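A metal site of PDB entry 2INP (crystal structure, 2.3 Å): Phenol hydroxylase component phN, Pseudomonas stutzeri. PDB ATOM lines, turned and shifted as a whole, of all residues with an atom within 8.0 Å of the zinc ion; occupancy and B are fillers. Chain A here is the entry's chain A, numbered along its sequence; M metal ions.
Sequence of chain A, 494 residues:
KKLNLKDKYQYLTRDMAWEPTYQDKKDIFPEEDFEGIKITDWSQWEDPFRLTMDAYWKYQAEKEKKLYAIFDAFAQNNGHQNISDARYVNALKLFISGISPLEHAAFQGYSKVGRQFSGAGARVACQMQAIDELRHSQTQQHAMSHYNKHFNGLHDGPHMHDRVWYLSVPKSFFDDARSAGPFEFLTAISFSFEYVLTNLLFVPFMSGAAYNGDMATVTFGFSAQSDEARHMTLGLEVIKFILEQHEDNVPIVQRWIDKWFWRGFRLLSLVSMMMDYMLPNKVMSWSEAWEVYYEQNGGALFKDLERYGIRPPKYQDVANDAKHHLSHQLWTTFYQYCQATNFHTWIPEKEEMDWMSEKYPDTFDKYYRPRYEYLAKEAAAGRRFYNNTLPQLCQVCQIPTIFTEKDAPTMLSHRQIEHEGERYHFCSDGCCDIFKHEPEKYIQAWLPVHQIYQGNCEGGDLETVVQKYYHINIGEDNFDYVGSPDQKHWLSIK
SG of Cys 397 lies close to N of Ile 399, 3.6 Å away. The backbone NH of Val 396 sits close to the side-chain sulfur of Cys 394 (3.6 Å). The guanidinium group of Arg 266 sits close to the side-chain sulfur of Cys 427. The side-chain hydroxyl of Ser 428 sits at hydrogen-bond distance from the backbone NH of Cys 431 (3.1 Å). The side-chain sulfur of Cys 431 lies close to the indole nitrogen of Trp 262, at 3.3 Å. The backbone carbonyl oxygen (O) of Ile 399 sits at hydrogen-bond distance from the backbone NH (N) of Cys 394. SG of Cys 427 lies close to OG of Ser 428.
Along chain A the residues within 4 Å of the zinc ion span positions 394 to 431.
The side-chain sulfur (SG) of Cys 394 is bound to the zinc ion (2.3 Å). The side-chain sulfur (SG) of Cys 397 binds the zinc ion, 2.3 Å away. The zinc ion is bound by SG of Cys 431 (2.3 Å). SG of Cys 427 is bound to the zinc ion. The zinc ion has four donor atoms within binding distance.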
ATOM      1  N   TRP A 262      -5.938 -13.700 -24.646  1.00  0.00           N
ATOM      2  CA  TRP A 262      -6.606 -12.717 -25.468  1.00  0.00           C
ATOM      3  C   TRP A 262      -5.815 -12.327 -26.724  1.00  0.00           C
ATOM      4  O   TRP A 262      -6.390 -12.324 -27.815  1.00  0.00           O
ATOM      5  CB  TRP A 262      -6.991 -11.467 -24.681  1.00  0.00           C
ATOM      6  CG  TRP A 262      -7.987 -10.646 -25.461  1.00  0.00           C
ATOM      7  CD1 TRP A 262      -7.761  -9.464 -26.163  1.00  0.00           C
ATOM      8  CD2 TRP A 262      -9.362 -10.972 -25.657  1.00  0.00           C
ATOM      9  NE1 TRP A 262      -8.942  -9.057 -26.782  1.00  0.00           N
ATOM     10  CE2 TRP A 262      -9.929  -9.965 -26.491  1.00  0.00           C
ATOM     11  CE3 TRP A 262     -10.182 -12.045 -25.231  1.00  0.00           C
ATOM     12  CZ2 TRP A 262     -11.305  -9.991 -26.869  1.00  0.00           C
ATOM     13  CZ3 TRP A 262     -11.510 -12.097 -25.656  1.00  0.00           C
ATOM     14  CH2 TRP A 262     -12.065 -11.057 -26.448  1.00  0.00           C
ATOM     15  N   ARG A 263      -4.550 -11.944 -26.602  1.00  0.00           N
ATOM     16  CA  ARG A 263      -3.781 -11.631 -27.804  1.00  0.00           C
ATOM     17  C   ARG A 263      -3.701 -12.833 -28.821  1.00  0.00           C
ATOM     18  O   ARG A 263      -3.799 -12.625 -30.036  1.00  0.00           O
ATOM     19  CB  ARG A 263      -2.354 -11.147 -27.458  1.00  0.00           C
ATOM     20  CG  ARG A 263      -2.296  -9.629 -27.010  1.00  0.00           C
ATOM     21  CD  ARG A 263      -1.007  -8.997 -27.453  1.00  0.00           C
ATOM     22  NE  ARG A 263      -1.097  -8.699 -28.893  1.00  0.00           N
ATOM     23  CZ  ARG A 263      -0.384  -7.815 -29.582  1.00  0.00           C
ATOM     24  NH1 ARG A 263       0.542  -7.061 -28.990  1.00  0.00           N
ATOM     25  NH2 ARG A 263      -0.637  -7.647 -30.882  1.00  0.00           N
ATOM     26  N   ARG A 266      -7.001 -13.175 -30.667  1.00  0.00           N
ATOM     27  CA  ARG A 266      -7.145 -12.175 -31.717  1.00  0.00           C
ATOM     28  C   ARG A 266      -6.266 -12.482 -32.918  1.00  0.00           C
ATOM     29  O   ARG A 266      -6.660 -12.240 -34.057  1.00  0.00           O
ATOM     30  CB  ARG A 266      -6.858 -10.751 -31.168  1.00  0.00           C
ATOM     31  CG  ARG A 266      -7.974 -10.134 -30.328  1.00  0.00           C
ATOM     32  CD  ARG A 266      -9.136  -9.713 -31.317  1.00  0.00           C
ATOM     33  NE  ARG A 266     -10.285  -9.011 -30.720  1.00  0.00           N
ATOM     34  CZ  ARG A 266     -11.490  -9.570 -30.584  1.00  0.00           C
ATOM     35  NH1 ARG A 266     -11.663 -10.825 -30.969  1.00  0.00           N
ATOM     36  NH2 ARG A 266     -12.501  -8.895 -30.027  1.00  0.00           N
ATOM     37  N   LEU A 393      -8.228   0.989 -36.363  1.00  0.00           N
ATOM     38  CA  LEU A 393      -7.489  -0.216 -35.823  1.00  0.00           C
ATOM     39  C   LEU A 393      -7.514  -0.271 -34.282  1.00  0.00           C
ATOM     40  O   LEU A 393      -7.494   0.741 -33.610  1.00  0.00           O
ATOM     41  CB  LEU A 393      -6.045  -0.258 -36.335  1.00  0.00           C
ATOM     42  CG  LEU A 393      -5.817  -0.173 -37.852  1.00  0.00           C
ATOM     43  CD1 LEU A 393      -4.327  -0.248 -38.117  1.00  0.00           C
ATOM     44  CD2 LEU A 393      -6.626  -1.246 -38.658  1.00  0.00           C
ATOM     45  N   CYS A 394      -7.546  -1.473 -33.729  1.00  0.00           N
ATOM     46  CA  CYS A 394      -7.329  -1.641 -32.291  1.00  0.00           C
ATOM     47  C   CYS A 394      -5.876  -1.284 -31.878  1.00  0.00           C
ATOM     48  O   CYS A 394      -4.896  -1.693 -32.564  1.00  0.00           O
ATOM     49  CB  CYS A 394      -7.658  -3.075 -31.928  1.00  0.00           C
ATOM     50  SG  CYS A 394      -7.405  -3.355 -30.125  1.00  0.00           S
ATOM     51  N   GLN A 395      -5.722  -0.463 -30.812  1.00  0.00           N
ATOM     52  CA  GLN A 395      -4.385  -0.022 -30.377  1.00  0.00           C
ATOM     53  C   GLN A 395      -3.496  -1.202 -29.872  1.00  0.00           C
ATOM     54  O   GLN A 395      -2.275  -1.158 -29.982  1.00  0.00           O
ATOM     55  CB  GLN A 395      -4.478   1.100 -29.346  1.00  0.00           C
ATOM     56  CG  GLN A 395      -3.105   1.689 -28.935  1.00  0.00           C
ATOM     57  CD  GLN A 395      -2.581   2.598 -29.956  1.00  0.00           C
ATOM     58  OE1 GLN A 395      -1.312   2.708 -30.224  1.00  0.00           O
ATOM     59  NE2 GLN A 395      -3.510   3.271 -30.592  1.00  0.00           N
ATOM     60  N   VAL A 396      -4.121  -2.251 -29.337  1.00  0.00           N
ATOM     61  CA  VAL A 396      -3.437  -3.471 -28.926  1.00  0.00           C
ATOM     62  C   VAL A 396      -3.296  -4.560 -30.083  1.00  0.00           C
ATOM     63  O   VAL A 396      -2.200  -4.735 -30.634  1.00  0.00           O
ATOM     64  CB  VAL A 396      -4.054  -4.011 -27.622  1.00  0.00           C
ATOM     65  CG1 VAL A 396      -3.375  -5.352 -27.196  1.00  0.00           C
ATOM     66  CG2 VAL A 396      -3.863  -3.043 -26.549  1.00  0.00           C
ATOM     67  N   CYS A 397      -4.363  -5.254 -30.456  1.00  0.00           N
ATOM     68  CA  CYS A 397      -4.186  -6.326 -31.443  1.00  0.00           C
ATOM     69  C   CYS A 397      -3.947  -5.851 -32.877  1.00  0.00           C
ATOM     70  O   CYS A 397      -3.359  -6.596 -33.728  1.00  0.00           O
ATOM     71  CB  CYS A 397      -5.343  -7.277 -31.392  1.00  0.00           C
ATOM     72  SG  CYS A 397      -6.891  -6.656 -31.901  1.00  0.00           S
ATOM     73  N   GLN A 398      -4.363  -4.587 -33.104  1.00  0.00           N
ATOM     74  CA  GLN A 398      -4.177  -3.863 -34.369  1.00  0.00           C
ATOM     75  C   GLN A 398      -5.107  -4.348 -35.499  1.00  0.00           C
ATOM     76  O   GLN A 398      -4.914  -3.960 -36.665  1.00  0.00           O
ATOM     77  CB  GLN A 398      -2.736  -3.821 -34.812  1.00  0.00           C
ATOM     78  CG  GLN A 398      -1.753  -3.274 -33.713  1.00  0.00           C
ATOM     79  CD  GLN A 398      -0.402  -2.940 -34.270  1.00  0.00           C
ATOM     80  OE1 GLN A 398      -0.294  -2.838 -35.463  1.00  0.00           O
ATOM     81  NE2 GLN A 398       0.615  -2.760 -33.420  1.00  0.00           N
ATOM     82  N   ILE A 399      -6.059  -5.206 -35.140  1.00  0.00           N
ATOM     83  CA  ILE A 399      -7.101  -5.648 -36.069  1.00  0.00           C
ATOM     84  C   ILE A 399      -8.069  -4.454 -36.219  1.00  0.00           C
ATOM     85  O   ILE A 399      -8.251  -3.663 -35.265  1.00  0.00           O
ATOM     86  CB  ILE A 399      -7.814  -6.967 -35.649  1.00  0.00           C
ATOM     87  CG1 ILE A 399      -6.780  -8.108 -35.381  1.00  0.00           C
ATOM     88  CG2 ILE A 399      -8.812  -7.411 -36.756  1.00  0.00           C
ATOM     89  CD1 ILE A 399      -7.382  -9.549 -35.076  1.00  0.00           C
ATOM     90  N   PRO A 400      -8.579  -4.247 -37.457  1.00  0.00           N
ATOM     91  CA  PRO A 400      -9.678  -3.291 -37.584  1.00  0.00           C
ATOM     92  C   PRO A 400     -10.723  -3.603 -36.557  1.00  0.00           C
ATOM     93  O   PRO A 400     -10.952  -4.767 -36.288  1.00  0.00           O
ATOM     94  CB  PRO A 400     -10.215  -3.558 -38.983  1.00  0.00           C
ATOM     95  CG  PRO A 400      -9.110  -4.231 -39.733  1.00  0.00           C
ATOM     96  CD  PRO A 400      -8.167  -4.825 -38.756  1.00  0.00           C
ATOM     97  N   THR A 401     -11.377  -2.579 -36.005  1.00  0.00           N
ATOM     98  CA  THR A 401     -12.273  -2.771 -34.906  1.00  0.00           C
ATOM     99  C   THR A 401     -13.646  -3.295 -35.378  1.00  0.00           C
ATOM    100  O   THR A 401     -14.665  -2.610 -35.387  1.00  0.00           O
ATOM    101  CB  THR A 401     -12.404  -1.470 -34.051  1.00  0.00           C
ATOM    102  OG1 THR A 401     -12.777  -0.380 -34.897  1.00  0.00           O
ATOM    103  CG2 THR A 401     -11.072  -1.160 -33.285  1.00  0.00           C
ATOM    104  N   PHE A 403     -15.177  -6.197 -34.319  1.00  0.00           N
ATOM    105  CA  PHE A 403     -15.766  -7.153 -33.395  1.00  0.00           C
ATOM    106  C   PHE A 403     -16.969  -6.605 -32.657  1.00  0.00           C
ATOM    107  O   PHE A 403     -17.050  -5.381 -32.376  1.00  0.00           O
ATOM    108  CB  PHE A 403     -14.668  -7.640 -32.426  1.00  0.00           C
ATOM    109  CG  PHE A 403     -13.548  -8.252 -33.142  1.00  0.00           C
ATOM    110  CD1 PHE A 403     -12.298  -7.671 -33.130  1.00  0.00           C
ATOM    111  CD2 PHE A 403     -13.778  -9.382 -33.926  1.00  0.00           C
ATOM    112  CE1 PHE A 403     -11.247  -8.250 -33.852  1.00  0.00           C
ATOM    113  CE2 PHE A 403     -12.739  -9.992 -34.649  1.00  0.00           C
ATOM    114  CZ  PHE A 403     -11.468  -9.424 -34.603  1.00  0.00           C
ATOM    115  N   HIS A 425      -8.087   3.679 -28.980  1.00  0.00           N
ATOM    116  CA  HIS A 425      -9.305   2.889 -29.204  1.00  0.00           C
ATOM    117  C   HIS A 425      -9.008   1.416 -29.274  1.00  0.00           C
ATOM    118  O   HIS A 425      -7.918   1.044 -29.715  1.00  0.00           O
ATOM    119  CB  HIS A 425      -9.947   3.296 -30.525  1.00  0.00           C
ATOM    120  CG  HIS A 425     -10.288   4.746 -30.571  1.00  0.00           C
ATOM    121  ND1 HIS A 425     -11.559   5.208 -30.274  1.00  0.00           N
ATOM    122  CD2 HIS A 425      -9.510   5.833 -30.780  1.00  0.00           C
ATOM    123  CE1 HIS A 425     -11.547   6.533 -30.382  1.00  0.00           C
ATOM    124  NE2 HIS A 425     -10.325   6.926 -30.689  1.00  0.00           N
ATOM    125  N   PHE A 426      -9.987   0.609 -28.888  1.00  0.00           N
ATOM    126  CA  PHE A 426      -9.802  -0.838 -28.711  1.00  0.00           C
ATOM    127  C   PHE A 426     -11.016  -1.518 -29.301  1.00  0.00           C
ATOM    128  O   PHE A 426     -12.159  -0.938 -29.294  1.00  0.00           O
ATOM    129  CB  PHE A 426      -9.595  -1.222 -27.230  1.00  0.00           C
ATOM    130  CG  PHE A 426      -8.626  -0.284 -26.538  1.00  0.00           C
ATOM    131  CD1 PHE A 426      -7.277  -0.480 -26.667  1.00  0.00           C
ATOM    132  CD2 PHE A 426      -9.101   0.846 -25.889  1.00  0.00           C
ATOM    133  CE1 PHE A 426      -6.386   0.411 -26.146  1.00  0.00           C
ATOM    134  CE2 PHE A 426      -8.238   1.773 -25.356  1.00  0.00           C
ATOM    135  CZ  PHE A 426      -6.860   1.559 -25.470  1.00  0.00           C
ATOM    136  N   CYS A 427     -10.740  -2.704 -29.852  1.00  0.00           N
ATOM    137  CA  CYS A 427     -11.780  -3.586 -30.327  1.00  0.00           C
ATOM    138  C   CYS A 427     -12.592  -4.272 -29.264  1.00  0.00           C
ATOM    139  O   CYS A 427     -13.578  -4.959 -29.602  1.00  0.00           O
ATOM    140  CB  CYS A 427     -11.149  -4.674 -31.205  1.00  0.00           C
ATOM    141  SG  CYS A 427     -10.239  -5.925 -30.231  1.00  0.00           S
ATOM    142  N   SER A 428     -12.215  -4.148 -27.983  1.00  0.00           N
ATOM    143  CA  SER A 428     -12.816  -5.013 -26.929  1.00  0.00           C
ATOM    144  C   SER A 428     -12.352  -4.608 -25.535  1.00  0.00           C
ATOM    145  O   SER A 428     -11.459  -3.827 -25.420  1.00  0.00           O
ATOM    146  CB  SER A 428     -12.382  -6.459 -27.139  1.00  0.00           C
ATOM    147  OG  SER A 428     -10.963  -6.501 -27.160  1.00  0.00           O
ATOM    148  N   ASP A 429     -12.948  -5.181 -24.484  1.00  0.00           N
ATOM    149  CA  ASP A 429     -12.487  -5.014 -23.115  1.00  0.00           C
ATOM    150  C   ASP A 429     -11.152  -5.715 -22.907  1.00  0.00           C
ATOM    151  O   ASP A 429     -10.233  -5.132 -22.295  1.00  0.00           O
ATOM    152  CB  ASP A 429     -13.526  -5.577 -22.161  1.00  0.00           C
ATOM    153  CG  ASP A 429     -14.699  -4.646 -22.027  1.00  0.00           C
ATOM    154  OD1 ASP A 429     -14.436  -3.400 -21.977  1.00  0.00           O
ATOM    155  OD2 ASP A 429     -15.864  -5.116 -22.044  1.00  0.00           O
ATOM    156  N   GLY A 430     -11.059  -6.932 -23.481  1.00  0.00           N
ATOM    157  CA  GLY A 430      -9.828  -7.670 -23.623  1.00  0.00           C
ATOM    158  C   GLY A 430      -8.627  -6.857 -23.959  1.00  0.00           C
ATOM    159  O   GLY A 430      -7.619  -6.959 -23.286  1.00  0.00           O
ATOM    160  N   CYS A 431      -8.683  -6.098 -25.035  1.00  0.00           N
ATOM    161  CA  CYS A 431      -7.519  -5.359 -25.483  1.00  0.00           C
ATOM    162  C   CYS A 431      -7.359  -4.025 -24.693  1.00  0.00           C
ATOM    163  O   CYS A 431      -6.255  -3.505 -24.479  1.00  0.00           O
ATOM    164  CB  CYS A 431      -7.641  -5.064 -26.972  1.00  0.00           C
ATOM    165  SG  CYS A 431      -7.342  -6.449 -28.050  1.00  0.00           S
ATOM    166  N   CYS A 432      -8.501  -3.475 -24.291  1.00  0.00           N
ATOM    167  CA  CYS A 432      -8.537  -2.322 -23.397  1.00  0.00           C
ATOM    168  C   CYS A 432      -7.818  -2.600 -22.055  1.00  0.00           C
ATOM    169  O   CYS A 432      -6.928  -1.840 -21.693  1.00  0.00           O
ATOM    170  CB  CYS A 432      -9.970  -1.869 -23.152  1.00  0.00           C
ATOM    171  SG  CYS A 432     -10.048  -0.363 -22.235  1.00  0.00           S
ATOM    172  N   ILE A 434      -5.563  -4.772 -21.508  1.00  0.00           N
ATOM    173  CA  ILE A 434      -4.151  -5.017 -21.761  1.00  0.00           C
ATOM    174  C   ILE A 434      -3.457  -3.677 -21.863  1.00  0.00           C
ATOM    175  O   ILE A 434      -2.368  -3.471 -21.306  1.00  0.00           O
ATOM    176  CB  ILE A 434      -3.873  -5.904 -23.026  1.00  0.00           C
ATOM    177  CG1 ILE A 434      -4.158  -7.397 -22.751  1.00  0.00           C
ATOM    178  CG2 ILE A 434      -2.477  -5.716 -23.510  1.00  0.00           C
ATOM    179  CD1 ILE A 434      -4.332  -8.338 -23.979  1.00  0.00           C
HETATM  180 ZN    ZN M   1      -7.924  -5.559 -30.131  1.00  0.00          ZN
